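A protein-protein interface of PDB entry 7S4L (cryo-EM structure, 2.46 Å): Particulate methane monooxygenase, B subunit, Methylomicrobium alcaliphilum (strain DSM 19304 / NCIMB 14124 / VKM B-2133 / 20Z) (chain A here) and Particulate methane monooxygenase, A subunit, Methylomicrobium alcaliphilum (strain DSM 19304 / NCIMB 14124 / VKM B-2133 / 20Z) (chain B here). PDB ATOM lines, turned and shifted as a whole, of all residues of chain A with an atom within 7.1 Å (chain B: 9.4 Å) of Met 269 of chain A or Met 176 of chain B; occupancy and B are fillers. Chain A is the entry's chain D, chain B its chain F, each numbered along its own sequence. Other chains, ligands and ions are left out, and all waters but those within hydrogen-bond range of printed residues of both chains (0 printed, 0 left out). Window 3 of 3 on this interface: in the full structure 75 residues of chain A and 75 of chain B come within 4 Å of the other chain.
OE1 of Glu 195 of chain B lies within hydrogen-bond range of N of Ser 113 of chain A (3.1 Å).
The backbone carbonyl oxygen of Gly 267 of chain A lies within hydrogen-bond range of the guanidinium group of Arg 112 of chain A, at 2.8 Å. The backbone carbonyl oxygen (O) of Ser 113 of chain A lies within hydrogen-bond range of the backbone NH (N) of Met 269 of chain A, at 2.9 Å. The backbone NH (N) of Val 171 of chain B is in hydrogen-bond range of the backbone carbonyl oxygen (O) of Met 178 of chain B (2.6 Å).
Among the printed residues, merely in contact across the chains: Leu 109 of chain A with Tyr 173 of chain B, Leu 109 of chain A with Asn 174 of chain B, Pro 111 of chain A with Met 176 of chain B, Pro 111 of chain A with Met 178 of chain B, Pro 111 of chain A with Tyr 186 of chain B, Arg 112 of chain A with Glu 195 of chain B and Met 269 of chain A with Met 176 of chain B.
Of the printed residues of chain B, Ser 113 of chain A touches Glu 195. Met 269 of chain A touches one residue of chain B. No residue of chain B comes within 4 Å of Gly 271 of chain A. Ile 272 of chain A touches none of the printed residues of chain B. Printed residues of chain A within 4 Å of Tyr 173 of chain B: Leu 109 (3.8 Å). Gly 175 of chain B touches none of the printed residues of chain A. The nearest residue of chain B that does not touch Met 269 of chain A is Glu 195 of chain B (7.4 Å). The nearest residue of chain A that does not touch Met 176 of chain B is Leu 109 of chain A (4.1 Å).
Hydrophobic or aromatic side chains of chain B that line the printed part of chain A: Met 176, Met 178 and Tyr 186. Of the 16 printed residues of chain A, 5 touch a printed residue of chain B. Hydrophobic or aromatic side chains of chain A that line the printed part of chain B: Leu 109, Pro 111 and Met 269. Along chain A the printed residues that touch a printed residue of chain B span positions 109 to 269. Among the printed residues, 8 pairs touch across the chains. Among the printed residues, no Asp or Glu carboxylate lies within 4 Å of a Lys or Arg side-chain nitrogen of the other chain.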
ATOM      1  N   GLU A  85       4.960  17.708 -27.270  1.00  0.00           N
ATOM      2  CA  GLU A  85       4.162  18.053 -26.098  1.00  0.00           C
ATOM      3  C   GLU A  85       4.383  17.047 -24.984  1.00  0.00           C
ATOM      4  O   GLU A  85       4.405  17.411 -23.803  1.00  0.00           O
ATOM      5  CB  GLU A  85       2.676  18.111 -26.447  1.00  0.00           C
ATOM      6  CG  GLU A  85       2.195  19.384 -27.111  1.00  0.00           C
ATOM      7  CD  GLU A  85       3.051  19.797 -28.278  1.00  0.00           C
ATOM      8  OE1 GLU A  85       3.559  18.900 -28.979  1.00  0.00           O
ATOM      9  OE2 GLU A  85       3.203  21.013 -28.507  1.00  0.00           O
ATOM     10  N   GLN A 108      14.814  19.531 -11.953  1.00  0.00           N
ATOM     11  CA  GLN A 108      13.645  18.866 -11.397  1.00  0.00           C
ATOM     12  C   GLN A 108      13.658  17.390 -11.752  1.00  0.00           C
ATOM     13  O   GLN A 108      13.987  17.019 -12.883  1.00  0.00           O
ATOM     14  CB  GLN A 108      12.354  19.491 -11.921  1.00  0.00           C
ATOM     15  CG  GLN A 108      12.284  20.986 -11.789  1.00  0.00           C
ATOM     16  CD  GLN A 108      11.008  21.542 -12.375  1.00  0.00           C
ATOM     17  OE1 GLN A 108      10.868  22.747 -12.560  1.00  0.00           O
ATOM     18  NE2 GLN A 108      10.063  20.658 -12.668  1.00  0.00           N
ATOM     19  N   LEU A 109      13.292  16.551 -10.793  1.00  0.00           N
ATOM     20  CA  LEU A 109      13.124  15.136 -11.079  1.00  0.00           C
ATOM     21  C   LEU A 109      12.004  14.945 -12.087  1.00  0.00           C
ATOM     22  O   LEU A 109      10.959  15.591 -11.996  1.00  0.00           O
ATOM     23  CB  LEU A 109      12.811  14.377  -9.795  1.00  0.00           C
ATOM     24  CG  LEU A 109      13.074  12.881  -9.861  1.00  0.00           C
ATOM     25  CD1 LEU A 109      14.503  12.602  -9.478  1.00  0.00           C
ATOM     26  CD2 LEU A 109      12.125  12.138  -8.957  1.00  0.00           C
ATOM     27  N   VAL A 110      12.214  14.058 -13.051  1.00  0.00           N
ATOM     28  CA  VAL A 110      11.226  13.863 -14.104  1.00  0.00           C
ATOM     29  C   VAL A 110      10.854  12.389 -14.214  1.00  0.00           C
ATOM     30  O   VAL A 110      11.129  11.760 -15.242  1.00  0.00           O
ATOM     31  CB  VAL A 110      11.737  14.390 -15.451  1.00  0.00           C
ATOM     32  CG1 VAL A 110      11.702  15.896 -15.463  1.00  0.00           C
ATOM     33  CG2 VAL A 110      13.131  13.888 -15.713  1.00  0.00           C
ATOM     34  N   PRO A 111      10.236  11.799 -13.195  1.00  0.00           N
ATOM     35  CA  PRO A 111       9.760  10.420 -13.338  1.00  0.00           C
ATOM     36  C   PRO A 111       8.584  10.293 -14.280  1.00  0.00           C
ATOM     37  O   PRO A 111       8.310   9.187 -14.754  1.00  0.00           O
ATOM     38  CB  PRO A 111       9.377  10.034 -11.910  1.00  0.00           C
ATOM     39  CG  PRO A 111       9.049  11.315 -11.264  1.00  0.00           C
ATOM     40  CD  PRO A 111       9.964  12.337 -11.855  1.00  0.00           C
ATOM     41  N   ARG A 112       7.875  11.377 -14.563  1.00  0.00           N
ATOM     42  CA  ARG A 112       6.770  11.360 -15.500  1.00  0.00           C
ATOM     43  C   ARG A 112       7.227  11.909 -16.843  1.00  0.00           C
ATOM     44  O   ARG A 112       8.378  12.304 -17.024  1.00  0.00           O
ATOM     45  CB  ARG A 112       5.595  12.175 -14.962  1.00  0.00           C
ATOM     46  CG  ARG A 112       5.520  12.250 -13.460  1.00  0.00           C
ATOM     47  CD  ARG A 112       4.610  11.181 -12.905  1.00  0.00           C
ATOM     48  NE  ARG A 112       4.103  11.540 -11.588  1.00  0.00           N
ATOM     49  CZ  ARG A 112       3.181  12.471 -11.381  1.00  0.00           C
ATOM     50  NH1 ARG A 112       2.671  13.134 -12.407  1.00  0.00           N
ATOM     51  NH2 ARG A 112       2.771  12.743 -10.153  1.00  0.00           N
ATOM     52  N   SER A 113       6.312  11.937 -17.799  1.00  0.00           N
ATOM     53  CA  SER A 113       6.606  12.591 -19.058  1.00  0.00           C
ATOM     54  C   SER A 113       6.623  14.101 -18.863  1.00  0.00           C
ATOM     55  O   SER A 113       6.150  14.625 -17.855  1.00  0.00           O
ATOM     56  CB  SER A 113       5.583  12.203 -20.115  1.00  0.00           C
ATOM     57  OG  SER A 113       4.283  12.185 -19.565  1.00  0.00           O
ATOM     58  N   VAL A 114       7.185  14.802 -19.842  1.00  0.00           N
ATOM     59  CA  VAL A 114       7.366  16.245 -19.766  1.00  0.00           C
ATOM     60  C   VAL A 114       7.021  16.859 -21.114  1.00  0.00           C
ATOM     61  O   VAL A 114       6.792  16.163 -22.102  1.00  0.00           O
ATOM     62  CB  VAL A 114       8.798  16.627 -19.361  1.00  0.00           C
ATOM     63  CG1 VAL A 114       9.160  15.966 -18.061  1.00  0.00           C
ATOM     64  CG2 VAL A 114       9.758  16.217 -20.440  1.00  0.00           C
ATOM     65  N   SER A 115       6.987  18.184 -21.142  1.00  0.00           N
ATOM     66  CA  SER A 115       6.704  18.948 -22.345  1.00  0.00           C
ATOM     67  C   SER A 115       7.924  19.765 -22.736  1.00  0.00           C
ATOM     68  O   SER A 115       8.651  20.261 -21.874  1.00  0.00           O
ATOM     69  CB  SER A 115       5.512  19.876 -22.134  1.00  0.00           C
ATOM     70  OG  SER A 115       4.299  19.210 -22.412  1.00  0.00           O
ATOM     71  N   LEU A 116       8.146  19.904 -24.036  1.00  0.00           N
ATOM     72  CA  LEU A 116       9.269  20.666 -24.549  1.00  0.00           C
ATOM     73  C   LEU A 116       8.778  21.641 -25.608  1.00  0.00           C
ATOM     74  O   LEU A 116       7.695  21.467 -26.171  1.00  0.00           O
ATOM     75  CB  LEU A 116      10.331  19.736 -25.125  1.00  0.00           C
ATOM     76  CG  LEU A 116      10.800  18.643 -24.166  1.00  0.00           C
ATOM     77  CD1 LEU A 116      11.841  17.778 -24.827  1.00  0.00           C
ATOM     78  CD2 LEU A 116      11.343  19.242 -22.890  1.00  0.00           C
ATOM     79  N   GLY A 267       0.896  11.265 -14.805  1.00  0.00           N
ATOM     80  CA  GLY A 267       0.517  12.594 -15.231  1.00  0.00           C
ATOM     81  C   GLY A 267       1.659  13.433 -15.748  1.00  0.00           C
ATOM     82  O   GLY A 267       2.737  13.478 -15.151  1.00  0.00           O
ATOM     83  N   LEU A 268       1.422  14.117 -16.862  1.00  0.00           N
ATOM     84  CA  LEU A 268       2.409  14.985 -17.486  1.00  0.00           C
ATOM     85  C   LEU A 268       2.947  16.015 -16.507  1.00  0.00           C
ATOM     86  O   LEU A 268       2.307  16.311 -15.497  1.00  0.00           O
ATOM     87  CB  LEU A 268       1.789  15.678 -18.695  1.00  0.00           C
ATOM     88  CG  LEU A 268       2.685  16.557 -19.549  1.00  0.00           C
ATOM     89  CD1 LEU A 268       3.701  15.708 -20.261  1.00  0.00           C
ATOM     90  CD2 LEU A 268       1.844  17.313 -20.543  1.00  0.00           C
ATOM     91  N   MET A 269       4.159  16.507 -16.783  1.00  0.00           N
ATOM     92  CA  MET A 269       4.780  17.589 -15.977  1.00  0.00           C
ATOM     93  C   MET A 269       5.107  18.713 -16.966  1.00  0.00           C
ATOM     94  O   MET A 269       6.264  18.772 -17.427  1.00  0.00           O
ATOM     95  CB  MET A 269       6.077  17.080 -15.345  1.00  0.00           C
ATOM     96  CG  MET A 269       6.618  17.951 -14.231  1.00  0.00           C
ATOM     97  SD  MET A 269       8.152  17.217 -13.629  1.00  0.00           S
ATOM     98  CE  MET A 269       7.898  15.524 -14.162  1.00  0.00           C
ATOM     99  N   ARG A 270       4.117  19.545 -17.312  1.00  0.00           N
ATOM    100  CA  ARG A 270       4.324  20.611 -18.331  1.00  0.00           C
ATOM    101  C   ARG A 270       5.441  21.562 -17.894  1.00  0.00           C
ATOM    102  O   ARG A 270       6.276  21.904 -18.751  1.00  0.00           O
ATOM    103  CB  ARG A 270       3.041  21.423 -18.541  1.00  0.00           C
ATOM    104  CG  ARG A 270       1.767  20.598 -18.630  1.00  0.00           C
ATOM    105  CD  ARG A 270       0.675  21.365 -19.353  1.00  0.00           C
ATOM    106  NE  ARG A 270       0.443  20.879 -20.705  1.00  0.00           N
ATOM    107  CZ  ARG A 270      -0.674  20.292 -21.117  1.00  0.00           C
ATOM    108  NH1 ARG A 270      -1.680  20.109 -20.278  1.00  0.00           N
ATOM    109  NH2 ARG A 270      -0.783  19.885 -22.369  1.00  0.00           N
ATOM    110  N   GLY A 271       5.444  21.978 -16.624  1.00  0.00           N
ATOM    111  CA  GLY A 271       6.442  22.952 -16.135  1.00  0.00           C
ATOM    112  C   GLY A 271       7.861  22.416 -16.173  1.00  0.00           C
ATOM    113  O   GLY A 271       8.281  21.801 -15.173  1.00  0.00           O
ATOM    114  N   ILE A 272       8.578  22.648 -17.277  1.00  0.00           N
ATOM    115  CA  ILE A 272      10.001  22.211 -17.396  1.00  0.00           C
ATOM    116  C   ILE A 272      10.819  23.431 -17.833  1.00  0.00           C
ATOM    117  O   ILE A 272      10.421  24.081 -18.822  1.00  0.00           O
ATOM    118  CB  ILE A 272      10.124  20.989 -18.332  1.00  0.00           C
ATOM    119  CG1 ILE A 272       9.899  19.689 -17.559  1.00  0.00           C
ATOM    120  CG2 ILE A 272      11.456  20.965 -19.057  1.00  0.00           C
ATOM    121  CD1 ILE A 272      10.797  19.534 -16.356  1.00  0.00           C
ATOM    122  N   PRO B 170       2.827   3.751  -0.539  1.00  0.00           N
ATOM    123  CA  PRO B 170       3.404   4.989  -1.059  1.00  0.00           C
ATOM    124  C   PRO B 170       4.845   5.167  -0.616  1.00  0.00           C
ATOM    125  O   PRO B 170       5.298   4.608   0.381  1.00  0.00           O
ATOM    126  CB  PRO B 170       2.507   6.073  -0.463  1.00  0.00           C
ATOM    127  CG  PRO B 170       1.981   5.469   0.767  1.00  0.00           C
ATOM    128  CD  PRO B 170       1.823   4.010   0.503  1.00  0.00           C
ATOM    129  N   VAL B 171       5.564   5.972  -1.390  1.00  0.00           N
ATOM    130  CA  VAL B 171       6.971   6.246  -1.133  1.00  0.00           C
ATOM    131  C   VAL B 171       7.276   7.649  -1.619  1.00  0.00           C
ATOM    132  O   VAL B 171       6.735   8.100  -2.630  1.00  0.00           O
ATOM    133  CB  VAL B 171       7.877   5.212  -1.829  1.00  0.00           C
ATOM    134  CG1 VAL B 171       9.290   5.709  -1.871  1.00  0.00           C
ATOM    135  CG2 VAL B 171       7.808   3.896  -1.106  1.00  0.00           C
ATOM    136  N   GLU B 172       8.136   8.347  -0.890  1.00  0.00           N
ATOM    137  CA  GLU B 172       8.627   9.650  -1.307  1.00  0.00           C
ATOM    138  C   GLU B 172      10.019   9.460  -1.883  1.00  0.00           C
ATOM    139  O   GLU B 172      10.946   9.072  -1.169  1.00  0.00           O
ATOM    140  CB  GLU B 172       8.655  10.637  -0.147  1.00  0.00           C
ATOM    141  CG  GLU B 172       9.307  11.946  -0.513  1.00  0.00           C
ATOM    142  CD  GLU B 172       9.542  12.830   0.684  1.00  0.00           C
ATOM    143  OE1 GLU B 172       9.529  12.312   1.818  1.00  0.00           O
ATOM    144  OE2 GLU B 172       9.739  14.047   0.494  1.00  0.00           O
ATOM    145  N   TYR B 173      10.164   9.730  -3.173  1.00  0.00           N
ATOM    146  CA  TYR B 173      11.414   9.504  -3.883  1.00  0.00           C
ATOM    147  C   TYR B 173      11.886  10.830  -4.453  1.00  0.00           C
ATOM    148  O   TYR B 173      11.275  11.362  -5.384  1.00  0.00           O
ATOM    149  CB  TYR B 173      11.229   8.470  -4.987  1.00  0.00           C
ATOM    150  CG  TYR B 173      12.519   7.888  -5.487  1.00  0.00           C
ATOM    151  CD1 TYR B 173      13.211   6.957  -4.739  1.00  0.00           C
ATOM    152  CD2 TYR B 173      13.045   8.270  -6.702  1.00  0.00           C
ATOM    153  CE1 TYR B 173      14.386   6.424  -5.187  1.00  0.00           C
ATOM    154  CE2 TYR B 173      14.223   7.742  -7.159  1.00  0.00           C
ATOM    155  CZ  TYR B 173      14.887   6.820  -6.397  1.00  0.00           C
ATOM    156  OH  TYR B 173      16.066   6.286  -6.848  1.00  0.00           O
ATOM    157  N   ASN B 174      12.967  11.362  -3.897  1.00  0.00           N
ATOM    158  CA  ASN B 174      13.563  12.594  -4.398  1.00  0.00           C
ATOM    159  C   ASN B 174      12.530  13.712  -4.490  1.00  0.00           C
ATOM    160  O   ASN B 174      12.533  14.513  -5.424  1.00  0.00           O
ATOM    161  CB  ASN B 174      14.227  12.364  -5.751  1.00  0.00           C
ATOM    162  CG  ASN B 174      15.567  11.687  -5.630  1.00  0.00           C
ATOM    163  OD1 ASN B 174      16.375  12.037  -4.774  1.00  0.00           O
ATOM    164  ND2 ASN B 174      15.813  10.709  -6.487  1.00  0.00           N
ATOM    165  N   GLY B 175      11.631  13.763  -3.516  1.00  0.00           N
ATOM    166  CA  GLY B 175      10.669  14.835  -3.436  1.00  0.00           C
ATOM    167  C   GLY B 175       9.323  14.556  -4.065  1.00  0.00           C
ATOM    168  O   GLY B 175       8.361  15.268  -3.759  1.00  0.00           O
ATOM    169  N   MET B 176       9.215  13.561  -4.933  1.00  0.00           N
ATOM    170  CA  MET B 176       7.939  13.181  -5.515  1.00  0.00           C
ATOM    171  C   MET B 176       7.392  11.958  -4.795  1.00  0.00           C
ATOM    172  O   MET B 176       8.143  11.129  -4.279  1.00  0.00           O
ATOM    173  CB  MET B 176       8.075  12.889  -7.009  1.00  0.00           C
ATOM    174  CG  MET B 176       8.004  14.119  -7.885  1.00  0.00           C
ATOM    175  SD  MET B 176       7.250  13.786  -9.484  1.00  0.00           S
ATOM    176  CE  MET B 176       7.243  15.426 -10.197  1.00  0.00           C
ATOM    177  N   MET B 177       6.070  11.856  -4.759  1.00  0.00           N
ATOM    178  CA  MET B 177       5.400  10.716  -4.154  1.00  0.00           C
ATOM    179  C   MET B 177       5.139   9.668  -5.223  1.00  0.00           C
ATOM    180  O   MET B 177       4.653   9.993  -6.310  1.00  0.00           O
ATOM    181  CB  MET B 177       4.089  11.128  -3.494  1.00  0.00           C
ATOM    182  CG  MET B 177       3.627  10.158  -2.431  1.00  0.00           C
ATOM    183  SD  MET B 177       1.847   9.923  -2.412  1.00  0.00           S
ATOM    184  CE  MET B 177       1.630   8.921  -3.870  1.00  0.00           C
ATOM    185  N   MET B 178       5.462   8.417  -4.914  1.00  0.00           N
ATOM    186  CA  MET B 178       5.293   7.331  -5.864  1.00  0.00           C
ATOM    187  C   MET B 178       4.987   6.054  -5.107  1.00  0.00           C
ATOM    188  O   MET B 178       5.454   5.856  -3.984  1.00  0.00           O
ATOM    189  CB  MET B 178       6.541   7.133  -6.725  1.00  0.00           C
ATOM    190  CG  MET B 178       7.114   8.408  -7.289  1.00  0.00           C
ATOM    191  SD  MET B 178       8.799   8.203  -7.877  1.00  0.00           S
ATOM    192  CE  MET B 178       8.516   7.155  -9.290  1.00  0.00           C
ATOM    193  N   THR B 179       4.196   5.190  -5.728  1.00  0.00           N
ATOM    194  CA  THR B 179       4.005   3.856  -5.200  1.00  0.00           C
ATOM    195  C   THR B 179       5.192   2.977  -5.565  1.00  0.00           C
ATOM    196  O   THR B 179       5.963   3.280  -6.474  1.00  0.00           O
ATOM    197  CB  THR B 179       2.715   3.251  -5.738  1.00  0.00           C
ATOM    198  OG1 THR B 179       2.744   3.274  -7.165  1.00  0.00           O
ATOM    199  CG2 THR B 179       1.527   4.045  -5.267  1.00  0.00           C
ATOM    200  N   ASP B 182       5.216   2.223  -9.227  1.00  0.00           N
ATOM    201  CA  ASP B 182       5.777   3.302 -10.029  1.00  0.00           C
ATOM    202  C   ASP B 182       7.284   3.358  -9.881  1.00  0.00           C
ATOM    203  O   ASP B 182       8.003   3.587 -10.854  1.00  0.00           O
ATOM    204  CB  ASP B 182       5.161   4.639  -9.628  1.00  0.00           C
ATOM    205  CG  ASP B 182       3.671   4.649  -9.770  1.00  0.00           C
ATOM    206  OD1 ASP B 182       3.039   3.631  -9.428  1.00  0.00           O
ATOM    207  OD2 ASP B 182       3.124   5.672 -10.220  1.00  0.00           O
ATOM    208  N   LEU B 183       7.785   3.144  -8.668  1.00  0.00           N
ATOM    209  CA  LEU B 183       9.224   3.137  -8.476  1.00  0.00           C
ATOM    210  C   LEU B 183       9.881   2.021  -9.269  1.00  0.00           C
ATOM    211  O   LEU B 183      10.942   2.228  -9.862  1.00  0.00           O
ATOM    212  CB  LEU B 183       9.552   3.002  -6.997  1.00  0.00           C
ATOM    213  CG  LEU B 183      10.955   3.462  -6.648  1.00  0.00           C
ATOM    214  CD1 LEU B 183      11.196   4.804  -7.274  1.00  0.00           C
ATOM    215  CD2 LEU B 183      11.115   3.533  -5.157  1.00  0.00           C
ATOM    216  N   TYR B 186      10.081   2.951 -12.769  1.00  0.00           N
ATOM    217  CA  TYR B 186      11.060   4.009 -12.959  1.00  0.00           C
ATOM    218  C   TYR B 186      12.480   3.466 -12.961  1.00  0.00           C
ATOM    219  O   TYR B 186      13.309   3.892 -13.765  1.00  0.00           O
ATOM    220  CB  TYR B 186      10.894   5.055 -11.863  1.00  0.00           C
ATOM    221  CG  TYR B 186      11.742   6.280 -12.035  1.00  0.00           C
ATOM    222  CD1 TYR B 186      11.710   7.006 -13.207  1.00  0.00           C
ATOM    223  CD2 TYR B 186      12.559   6.722 -11.015  1.00  0.00           C
ATOM    224  CE1 TYR B 186      12.476   8.127 -13.362  1.00  0.00           C
ATOM    225  CE2 TYR B 186      13.328   7.842 -11.162  1.00  0.00           C
ATOM    226  CZ  TYR B 186      13.281   8.542 -12.339  1.00  0.00           C
ATOM    227  OH  TYR B 186      14.047   9.664 -12.494  1.00  0.00           O
ATOM    228  N   GLU B 195       7.195   6.221 -20.659  1.00  0.00           N
ATOM    229  CA  GLU B 195       6.191   6.335 -19.611  1.00  0.00           C
ATOM    230  C   GLU B 195       4.854   6.806 -20.167  1.00  0.00           C
ATOM    231  O   GLU B 195       3.797   6.436 -19.648  1.00  0.00           O
ATOM    232  CB  GLU B 195       6.674   7.280 -18.521  1.00  0.00           C
ATOM    233  CG  GLU B 195       5.914   7.135 -17.223  1.00  0.00           C
ATOM    234  CD  GLU B 195       4.735   8.071 -17.131  1.00  0.00           C
ATOM    235  OE1 GLU B 195       4.817   9.199 -17.656  1.00  0.00           O
ATOM    236  OE2 GLU B 195       3.716   7.673 -16.535  1.00  0.00           O
ATOM    237  N   TYR B 196       4.876   7.623 -21.218  1.00  0.00           N
ATOM    238  CA  TYR B 196       3.637   8.227 -21.686  1.00  0.00           C
ATOM    239  C   TYR B 196       2.701   7.226 -22.344  1.00  0.00           C
ATOM    240  O   TYR B 196       1.496   7.480 -22.399  1.00  0.00           O
ATOM    241  CB  TYR B 196       3.929   9.374 -22.651  1.00  0.00           C
ATOM    242  CG  TYR B 196       4.723   8.980 -23.866  1.00  0.00           C
ATOM    243  CD1 TYR B 196       4.116   8.345 -24.932  1.00  0.00           C
ATOM    244  CD2 TYR B 196       6.073   9.251 -23.948  1.00  0.00           C
ATOM    245  CE1 TYR B 196       4.832   7.984 -26.038  1.00  0.00           C
ATOM    246  CE2 TYR B 196       6.796   8.893 -25.053  1.00  0.00           C
ATOM    247  CZ  TYR B 196       6.171   8.260 -26.097  1.00  0.00           C
ATOM    248  OH  TYR B 196       6.884   7.897 -27.211  1.00  0.00           O
